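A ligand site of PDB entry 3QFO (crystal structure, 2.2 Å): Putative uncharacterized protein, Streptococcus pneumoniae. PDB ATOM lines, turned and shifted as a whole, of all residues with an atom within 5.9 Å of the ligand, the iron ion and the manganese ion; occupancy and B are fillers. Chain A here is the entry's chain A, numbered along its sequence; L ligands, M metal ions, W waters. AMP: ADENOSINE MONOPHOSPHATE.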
ATOM      1  N   ASP A  19     -16.058 -14.270 -35.255  1.00  0.00           N
ATOM      2  CA  ASP A  19     -15.126 -13.985 -34.155  1.00  0.00           C
ATOM      3  C   ASP A  19     -14.267 -15.219 -33.827  1.00  0.00           C
ATOM      4  O   ASP A  19     -14.211 -15.685 -32.679  1.00  0.00           O
ATOM      5  CB  ASP A  19     -15.913 -13.488 -32.935  1.00  0.00           C
ATOM      6  CG  ASP A  19     -16.629 -12.161 -33.201  1.00  0.00           C
ATOM      7  OD1 ASP A  19     -17.893 -12.145 -33.265  1.00  0.00           O
ATOM      8  OD2 ASP A  19     -15.906 -11.141 -33.366  1.00  0.00           O
ATOM      9  N   HIS A  21     -10.946 -15.185 -34.365  1.00  0.00           N
ATOM     10  CA  HIS A  21      -9.798 -14.553 -33.722  1.00  0.00           C
ATOM     11  C   HIS A  21      -8.556 -15.433 -33.702  1.00  0.00           C
ATOM     12  O   HIS A  21      -7.846 -15.491 -32.703  1.00  0.00           O
ATOM     13  CB  HIS A  21     -10.158 -14.109 -32.304  1.00  0.00           C
ATOM     14  CG  HIS A  21     -11.018 -12.879 -32.257  1.00  0.00           C
ATOM     15  ND1 HIS A  21     -10.496 -11.605 -32.341  1.00  0.00           N
ATOM     16  CD2 HIS A  21     -12.362 -12.742 -32.153  1.00  0.00           C
ATOM     17  CE1 HIS A  21     -11.479 -10.726 -32.267  1.00  0.00           C
ATOM     18  NE2 HIS A  21     -12.620 -11.389 -32.168  1.00  0.00           N
ATOM     19  N   GLY A  46     -16.877 -12.168 -39.608  1.00  0.00           N
ATOM     20  CA  GLY A  46     -15.651 -11.377 -39.405  1.00  0.00           C
ATOM     21  C   GLY A  46     -14.948 -11.561 -38.063  1.00  0.00           C
ATOM     22  O   GLY A  46     -15.409 -12.340 -37.193  1.00  0.00           O
ATOM     23  N   ASP A  47     -13.856 -10.818 -37.891  1.00  0.00           N
ATOM     24  CA  ASP A  47     -12.856 -11.041 -36.832  1.00  0.00           C
ATOM     25  C   ASP A  47     -12.260 -12.438 -36.973  1.00  0.00           C
ATOM     26  O   ASP A  47     -12.437 -13.327 -36.142  1.00  0.00           O
ATOM     27  CB  ASP A  47     -13.398 -10.739 -35.429  1.00  0.00           C
ATOM     28  CG  ASP A  47     -13.616  -9.250 -35.189  1.00  0.00           C
ATOM     29  OD1 ASP A  47     -13.351  -8.450 -36.123  1.00  0.00           O
ATOM     30  OD2 ASP A  47     -14.069  -8.853 -34.092  1.00  0.00           O
ATOM     31  N   GLY A  73     -15.162  -7.478 -40.269  1.00  0.00           N
ATOM     32  CA  GLY A  73     -15.048  -7.218 -38.834  1.00  0.00           C
ATOM     33  C   GLY A  73     -14.031  -6.123 -38.548  1.00  0.00           C
ATOM     34  O   GLY A  73     -13.199  -5.811 -39.393  1.00  0.00           O
ATOM     35  N   ASN A  74     -14.087  -5.539 -37.348  1.00  0.00           N
ATOM     36  CA  ASN A  74     -13.137  -4.479 -36.986  1.00  0.00           C
ATOM     37  C   ASN A  74     -11.677  -4.953 -36.870  1.00  0.00           C
ATOM     38  O   ASN A  74     -10.755  -4.144 -37.035  1.00  0.00           O
ATOM     39  CB  ASN A  74     -13.569  -3.806 -35.700  1.00  0.00           C
ATOM     40  CG  ASN A  74     -13.828  -4.812 -34.584  1.00  0.00           C
ATOM     41  OD1 ASN A  74     -14.459  -5.838 -34.808  1.00  0.00           O
ATOM     42  ND2 ASN A  74     -13.304  -4.535 -33.408  1.00  0.00           N
ATOM     43  N   TRP A  75     -11.465  -6.242 -36.584  1.00  0.00           N
ATOM     44  CA  TRP A  75     -10.109  -6.793 -36.529  1.00  0.00           C
ATOM     45  C   TRP A  75      -9.448  -6.945 -37.911  1.00  0.00           C
ATOM     46  O   TRP A  75      -8.223  -6.971 -38.004  1.00  0.00           O
ATOM     47  CB  TRP A  75     -10.038  -8.089 -35.713  1.00  0.00           C
ATOM     48  CG  TRP A  75     -10.067  -7.841 -34.216  1.00  0.00           C
ATOM     49  CD1 TRP A  75     -11.127  -7.380 -33.488  1.00  0.00           C
ATOM     50  CD2 TRP A  75      -9.008  -8.033 -33.277  1.00  0.00           C
ATOM     51  NE1 TRP A  75     -10.790  -7.247 -32.164  1.00  0.00           N
ATOM     52  CE2 TRP A  75      -9.496  -7.665 -32.004  1.00  0.00           C
ATOM     53  CE3 TRP A  75      -7.678  -8.476 -33.379  1.00  0.00           C
ATOM     54  CZ2 TRP A  75      -8.710  -7.724 -30.841  1.00  0.00           C
ATOM     55  CZ3 TRP A  75      -6.884  -8.528 -32.216  1.00  0.00           C
ATOM     56  CH2 TRP A  75      -7.409  -8.165 -30.965  1.00  0.00           C
ATOM     57  N   HIS A 136     -21.109  -7.251 -39.127  1.00  0.00           N
ATOM     58  CA  HIS A 136     -20.301  -7.611 -37.956  1.00  0.00           C
ATOM     59  C   HIS A 136     -20.916  -7.022 -36.696  1.00  0.00           C
ATOM     60  O   HIS A 136     -21.118  -7.716 -35.707  1.00  0.00           O
ATOM     61  CB  HIS A 136     -18.848  -7.148 -38.083  1.00  0.00           C
ATOM     62  CG  HIS A 136     -17.969  -7.596 -36.943  1.00  0.00           C
ATOM     63  ND1 HIS A 136     -17.647  -8.924 -36.750  1.00  0.00           N
ATOM     64  CD2 HIS A 136     -17.362  -6.903 -35.947  1.00  0.00           C
ATOM     65  CE1 HIS A 136     -16.866  -9.033 -35.681  1.00  0.00           C
ATOM     66  NE2 HIS A 136     -16.673  -7.818 -35.189  1.00  0.00           N
ATOM     67  N   ASN A 142     -18.396  -1.226 -37.757  1.00  0.00           N
ATOM     68  CA  ASN A 142     -18.088  -2.596 -37.311  1.00  0.00           C
ATOM     69  C   ASN A 142     -17.347  -2.675 -35.958  1.00  0.00           C
ATOM     70  O   ASN A 142     -16.815  -3.724 -35.589  1.00  0.00           O
ATOM     71  CB  ASN A 142     -17.339  -3.366 -38.401  1.00  0.00           C
ATOM     72  CG  ASN A 142     -15.948  -2.831 -38.646  1.00  0.00           C
ATOM     73  OD1 ASN A 142     -15.441  -1.990 -37.913  1.00  0.00           O
ATOM     74  ND2 ASN A 142     -15.299  -3.337 -39.675  1.00  0.00           N
ATOM     75  N   ARG A 145     -19.588  -0.410 -28.932  1.00  0.00           N
ATOM     76  CA  ARG A 145     -20.297  -1.110 -27.869  1.00  0.00           C
ATOM     77  C   ARG A 145     -21.791  -0.864 -27.938  1.00  0.00           C
ATOM     78  O   ARG A 145     -22.510  -1.198 -26.987  1.00  0.00           O
ATOM     79  CB  ARG A 145     -19.811  -0.642 -26.501  1.00  0.00           C
ATOM     80  CG  ARG A 145     -18.355  -0.904 -26.185  1.00  0.00           C
ATOM     81  CD  ARG A 145     -17.976  -2.380 -26.295  1.00  0.00           C
ATOM     82  NE  ARG A 145     -16.914  -2.707 -25.333  1.00  0.00           N
ATOM     83  CZ  ARG A 145     -15.867  -3.469 -25.607  1.00  0.00           C
ATOM     84  NH1 ARG A 145     -14.956  -3.694 -24.663  1.00  0.00           N
ATOM     85  NH2 ARG A 145     -15.709  -3.985 -26.824  1.00  0.00           N
ATOM     86  N   ILE A 148     -24.144  -4.162 -27.286  1.00  0.00           N
ATOM     87  CA  ILE A 148     -23.884  -5.047 -26.162  1.00  0.00           C
ATOM     88  C   ILE A 148     -25.204  -5.586 -25.577  1.00  0.00           C
ATOM     89  O   ILE A 148     -26.296  -5.124 -25.960  1.00  0.00           O
ATOM     90  CB  ILE A 148     -23.044  -4.373 -25.038  1.00  0.00           C
ATOM     91  CG1 ILE A 148     -23.730  -3.104 -24.500  1.00  0.00           C
ATOM     92  CG2 ILE A 148     -21.618  -4.126 -25.536  1.00  0.00           C
ATOM     93  CD1 ILE A 148     -23.019  -2.489 -23.259  1.00  0.00           C
ATOM     94  N   HIS A 149     -25.098  -6.532 -24.654  1.00  0.00           N
ATOM     95  CA  HIS A 149     -26.265  -7.189 -24.066  1.00  0.00           C
ATOM     96  C   HIS A 149     -27.302  -6.205 -23.507  1.00  0.00           C
ATOM     97  O   HIS A 149     -28.493  -6.471 -23.554  1.00  0.00           O
ATOM     98  CB  HIS A 149     -25.847  -8.253 -23.019  1.00  0.00           C
ATOM     99  CG  HIS A 149     -25.289  -7.696 -21.746  1.00  0.00           C
ATOM    100  ND1 HIS A 149     -24.300  -6.733 -21.721  1.00  0.00           N
ATOM    101  CD2 HIS A 149     -25.576  -7.966 -20.450  1.00  0.00           C
ATOM    102  CE1 HIS A 149     -24.017  -6.425 -20.467  1.00  0.00           C
ATOM    103  NE2 HIS A 149     -24.776  -7.161 -19.675  1.00  0.00           N
ATOM    104  N   THR A 150     -26.840  -5.056 -23.009  1.00  0.00           N
ATOM    105  CA  THR A 150     -27.736  -4.046 -22.441  1.00  0.00           C
ATOM    106  C   THR A 150     -27.911  -2.825 -23.345  1.00  0.00           C
ATOM    107  O   THR A 150     -28.343  -1.762 -22.885  1.00  0.00           O
ATOM    108  CB  THR A 150     -27.258  -3.587 -21.045  1.00  0.00           C
ATOM    109  OG1 THR A 150     -25.875  -3.242 -21.100  1.00  0.00           O
ATOM    110  CG2 THR A 150     -27.448  -4.690 -20.011  1.00  0.00           C
ATOM    111  N   HIS A 172     -19.507  -9.724 -33.157  1.00  0.00           N
ATOM    112  CA  HIS A 172     -18.814  -8.627 -32.455  1.00  0.00           C
ATOM    113  C   HIS A 172     -18.867  -8.646 -30.921  1.00  0.00           C
ATOM    114  O   HIS A 172     -17.881  -8.324 -30.264  1.00  0.00           O
ATOM    115  CB  HIS A 172     -19.247  -7.266 -32.994  1.00  0.00           C
ATOM    116  CG  HIS A 172     -18.473  -6.116 -32.452  1.00  0.00           C
ATOM    117  ND1 HIS A 172     -17.106  -5.966 -32.650  1.00  0.00           N
ATOM    118  CD2 HIS A 172     -18.866  -5.066 -31.681  1.00  0.00           C
ATOM    119  CE1 HIS A 172     -16.705  -4.860 -32.041  1.00  0.00           C
ATOM    120  NE2 HIS A 172     -17.740  -4.302 -31.458  1.00  0.00           N
ATOM    121  N   ILE A 173     -20.017  -8.986 -30.341  1.00  0.00           N
ATOM    122  CA  ILE A 173     -20.113  -8.956 -28.882  1.00  0.00           C
ATOM    123  C   ILE A 173     -19.692 -10.266 -28.206  1.00  0.00           C
ATOM    124  O   ILE A 173     -19.549 -10.303 -26.982  1.00  0.00           O
ATOM    125  CB  ILE A 173     -21.511  -8.504 -28.390  1.00  0.00           C
ATOM    126  CG1 ILE A 173     -22.595  -9.523 -28.787  1.00  0.00           C
ATOM    127  CG2 ILE A 173     -21.822  -7.086 -28.883  1.00  0.00           C
ATOM    128  CD1 ILE A 173     -23.890  -9.384 -27.989  1.00  0.00           C
ATOM    129  N   HIS A 174     -19.483 -11.324 -29.000  1.00  0.00           N
ATOM    130  CA  HIS A 174     -18.947 -12.588 -28.499  1.00  0.00           C
ATOM    131  C   HIS A 174     -19.928 -13.258 -27.528  1.00  0.00           C
ATOM    132  O   HIS A 174     -19.531 -13.959 -26.586  1.00  0.00           O
ATOM    133  CB  HIS A 174     -17.572 -12.374 -27.823  1.00  0.00           C
ATOM    134  CG  HIS A 174     -16.462 -12.030 -28.778  1.00  0.00           C
ATOM    135  ND1 HIS A 174     -15.166 -12.495 -28.613  1.00  0.00           N
ATOM    136  CD2 HIS A 174     -16.453 -11.298 -29.922  1.00  0.00           C
ATOM    137  CE1 HIS A 174     -14.415 -12.060 -29.610  1.00  0.00           C
ATOM    138  NE2 HIS A 174     -15.158 -11.321 -30.411  1.00  0.00           N
ATOM    139  N   GLN A 175     -21.217 -13.017 -27.759  1.00  0.00           N
ATOM    140  CA  GLN A 175     -22.294 -13.635 -26.985  1.00  0.00           C
ATOM    141  C   GLN A 175     -23.396 -14.126 -27.926  1.00  0.00           C
ATOM    142  O   GLN A 175     -23.710 -13.482 -28.913  1.00  0.00           O
ATOM    143  CB  GLN A 175     -22.918 -12.626 -26.012  1.00  0.00           C
ATOM    144  CG  GLN A 175     -21.991 -12.013 -24.954  1.00  0.00           C
ATOM    145  CD  GLN A 175     -22.815 -11.323 -23.889  1.00  0.00           C
ATOM    146  OE1 GLN A 175     -23.181 -10.154 -24.047  1.00  0.00           O
ATOM    147  NE2 GLN A 175     -23.200 -12.075 -22.848  1.00  0.00           N
ATOM    148  N   SER A 192     -19.008 -16.287 -30.278  1.00  0.00           N
ATOM    149  CA  SER A 192     -17.632 -16.321 -30.787  1.00  0.00           C
ATOM    150  C   SER A 192     -17.064 -17.739 -30.809  1.00  0.00           C
ATOM    151  O   SER A 192     -17.137 -18.467 -29.835  1.00  0.00           O
ATOM    152  CB  SER A 192     -16.748 -15.421 -29.894  1.00  0.00           C
ATOM    153  OG  SER A 192     -15.382 -15.510 -30.251  1.00  0.00           O
ATOM    154  N   GLN A 195     -13.132 -16.840 -28.878  1.00  0.00           N
ATOM    155  CA  GLN A 195     -13.014 -16.003 -27.688  1.00  0.00           C
ATOM    156  C   GLN A 195     -14.395 -15.796 -27.023  1.00  0.00           C
ATOM    157  O   GLN A 195     -14.812 -14.649 -26.842  1.00  0.00           O
ATOM    158  CB  GLN A 195     -12.440 -14.612 -28.022  1.00  0.00           C
ATOM    159  CG  GLN A 195     -11.051 -14.549 -28.711  1.00  0.00           C
ATOM    160  CD  GLN A 195      -9.900 -14.782 -27.738  1.00  0.00           C
ATOM    161  OE1 GLN A 195      -9.253 -13.827 -27.290  1.00  0.00           O
ATOM    162  NE2 GLN A 195      -9.663 -16.041 -27.387  1.00  0.00           N
ATOM    163  N   PHE A 197     -17.480 -15.002 -24.672  1.00  0.00           N
ATOM    164  CA  PHE A 197     -17.470 -13.969 -23.658  1.00  0.00           C
ATOM    165  C   PHE A 197     -18.671 -14.067 -22.749  1.00  0.00           C
ATOM    166  O   PHE A 197     -19.818 -14.112 -23.204  1.00  0.00           O
ATOM    167  CB  PHE A 197     -17.355 -12.573 -24.277  1.00  0.00           C
ATOM    168  CG  PHE A 197     -17.357 -11.453 -23.274  1.00  0.00           C
ATOM    169  CD1 PHE A 197     -16.261 -11.257 -22.417  1.00  0.00           C
ATOM    170  CD2 PHE A 197     -18.457 -10.599 -23.166  1.00  0.00           C
ATOM    171  CE1 PHE A 197     -16.263 -10.224 -21.453  1.00  0.00           C
ATOM    172  CE2 PHE A 197     -18.468  -9.554 -22.216  1.00  0.00           C
ATOM    173  CZ  PHE A 197     -17.370  -9.376 -21.360  1.00  0.00           C
ATOM    174  N   LEU A 199     -20.238 -12.504 -18.962  1.00  0.00           N
ATOM    175  CA  LEU A 199     -20.179 -11.616 -17.806  1.00  0.00           C
ATOM    176  C   LEU A 199     -20.509 -12.393 -16.532  1.00  0.00           C
ATOM    177  O   LEU A 199     -20.157 -11.975 -15.429  1.00  0.00           O
ATOM    178  CB  LEU A 199     -21.120 -10.407 -17.951  1.00  0.00           C
ATOM    179  CG  LEU A 199     -20.661  -9.288 -18.884  1.00  0.00           C
ATOM    180  CD1 LEU A 199     -21.208  -9.530 -20.264  1.00  0.00           C
ATOM    181  CD2 LEU A 199     -21.152  -7.930 -18.412  1.00  0.00           C
ATOM    182  N   HIS A 260     -10.953 -11.096 -20.361  1.00  0.00           N
ATOM    183  CA  HIS A 260     -10.402 -10.397 -21.531  1.00  0.00           C
ATOM    184  C   HIS A 260      -9.648  -9.114 -21.160  1.00  0.00           C
ATOM    185  O   HIS A 260     -10.222  -8.200 -20.558  1.00  0.00           O
ATOM    186  CB  HIS A 260     -11.500 -10.130 -22.574  1.00  0.00           C
ATOM    187  CG  HIS A 260     -12.082 -11.378 -23.196  1.00  0.00           C
ATOM    188  ND1 HIS A 260     -13.215 -11.348 -23.981  1.00  0.00           N
ATOM    189  CD2 HIS A 260     -11.687 -12.660 -23.150  1.00  0.00           C
ATOM    190  CE1 HIS A 260     -13.486 -12.572 -24.395  1.00  0.00           C
ATOM    191  NE2 HIS A 260     -12.572 -13.390 -23.908  1.00  0.00           N
HETATM  192  P   AMP L   1     -13.821  -7.286 -30.669  1.00  0.00           P
HETATM  193  O1P AMP L   1     -14.404  -6.566 -31.859  1.00  0.00           O
HETATM  194  O2P AMP L   1     -13.545  -8.749 -30.886  1.00  0.00           O
HETATM  195  O3P AMP L   1     -12.639  -6.539 -30.121  1.00  0.00           O
HETATM  196  O5' AMP L   1     -14.956  -7.174 -29.525  1.00  0.00           O
HETATM  197  C5' AMP L   1     -15.383  -8.277 -28.732  1.00  0.00           C
HETATM  198  C4' AMP L   1     -15.035  -8.062 -27.263  1.00  0.00           C
HETATM  199  O4' AMP L   1     -15.750  -6.968 -26.683  1.00  0.00           O
HETATM  200  C3' AMP L   1     -15.455  -9.249 -26.396  1.00  0.00           C
HETATM  201  O3' AMP L   1     -14.510 -10.320 -26.450  1.00  0.00           O
HETATM  202  C2' AMP L   1     -15.495  -8.647 -25.019  1.00  0.00           C
HETATM  203  O2' AMP L   1     -14.189  -8.719 -24.419  1.00  0.00           O
HETATM  204  C1' AMP L   1     -15.906  -7.206 -25.278  1.00  0.00           C
HETATM  205  N9  AMP L   1     -17.318  -7.058 -24.828  1.00  0.00           N
HETATM  206  C8  AMP L   1     -18.427  -7.498 -25.476  1.00  0.00           C
HETATM  207  N7  AMP L   1     -19.550  -7.203 -24.762  1.00  0.00           N
HETATM  208  C5  AMP L   1     -19.159  -6.564 -23.643  1.00  0.00           C
HETATM  209  C6  AMP L   1     -19.836  -5.992 -22.455  1.00  0.00           C
HETATM  210  N6  AMP L   1     -21.183  -6.042 -22.338  1.00  0.00           N
HETATM  211  N1  AMP L   1     -19.054  -5.425 -21.492  1.00  0.00           N
HETATM  212  C2  AMP L   1     -17.707  -5.375 -21.580  1.00  0.00           C
HETATM  213  N3  AMP L   1     -17.029  -5.882 -22.645  1.00  0.00           N
HETATM  214  C4  AMP L   1     -17.687  -6.475 -23.687  1.00  0.00           C
HETATM  215 FE    FE M   1     -14.471 -10.169 -32.176  1.00  0.00          FE
HETATM  216 MN    MN M   2     -15.470  -7.279 -33.496  1.00  0.00          MN
HETATM  217  O   HOH W   1     -15.678  -8.478 -31.927  1.00  0.00           O
HETATM  218  O   HOH W   2     -22.265  -7.645 -24.550  1.00  0.00           O
HETATM  219  O   HOH W   3     -11.934  -9.958 -28.592  1.00  0.00           O
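Of the 22 residues printed, 5 come within 4 Å of the manganese ion. Along chain A the residues within 4 Å of the manganese ion span positions 19 to 172. The nearest printed residue that does not touch the manganese ion is Asn 142 (4.3 Å).
The iron ion is bound by water W1 (2.1 Å), the side-chain carboxylate (OD2) of Asp 19 (2.1 Å), an oxygen (O2P) of the ligand (2.1 Å), a ring nitrogen (NE2) of His 21 (2.2 Å), a ring nitrogen (NE2) of His 174 (2.2 Å) and the side-chain carboxylate (OD2) of Asp 47 (2.4 Å).
Water W1 lies within hydrogen-bond range of O of His 172 and O5' of the ligand. Water W2 lies within hydrogen-bond range of OE1 of Gln 175 (2.7 Å), N7 of the ligand (2.8 Å) and N of His 149 (3.0 Å).
The manganese ion is bound by water W1 (2.0 Å), an oxygen (O1P) of the ligand (2.1 Å), a ring nitrogen (NE2) of His 136 (2.1 Å), the side-chain carboxylate (OD2) of Asp 47 (2.2 Å), the side-chain amide oxygen (OD1) of Asn 74 (2.2 Å) and a ring nitrogen (ND1) of His 172 (2.3 Å). The manganese ion has six donor atoms within binding distance.
Residues that only touch the ligand: Ile 173, Phe 197 and Ile 148. Hydrophobic or aromatic side chains that line the ligand: His 21, Trp 75, Ile 148, His 149, His 172, His 174, Phe 197 and His 260. Of the 22 residues printed, 12 come within 4 Å of the ligand.
NH2 of Arg 145 sits at hydrogen-bond distance from O4' of the ligand (3.0 Å). A ring nitrogen (ND1) of His 149 lies within hydrogen-bond range of a nitrogen (N6) of the ligand (3.3 Å). ND1 of His 260 sits at hydrogen-bond distance from O2' of the ligand (2.8 Å). NE1 of Trp 75 sits at hydrogen-bond distance from O3P of the ligand, 2.8 Å away.
Along chain A the residues within 4 Å of the iron ion span positions 19 to 174.
N of Trp 75 lies within hydrogen-bond range of OD1 of Asp 47 (2.9 Å). O of His 174 is in hydrogen-bond range of N of Phe 197 (3.0 Å). The backbone NH (N) of Asn 74 lies close to the side-chain amide nitrogen (ND2) of Asn 142 (3.4 Å). The backbone NH of Asp 19 is in hydrogen-bond range of the backbone carbonyl oxygen of Gly 46 (2.8 Å). A ring nitrogen (ND1) of His 174 lies within hydrogen-bond range of the side-chain hydroxyl (OG) of Ser 192. O of Gln 195 sits at hydrogen-bond distance from ND1 of His 174. The side-chain carboxylate of Asp 19 lies within hydrogen-bond range of the backbone NH of His 172 (2.9 Å). O of Asp 19 lies within hydrogen-bond range of OG of Ser 192 (2.7 Å).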
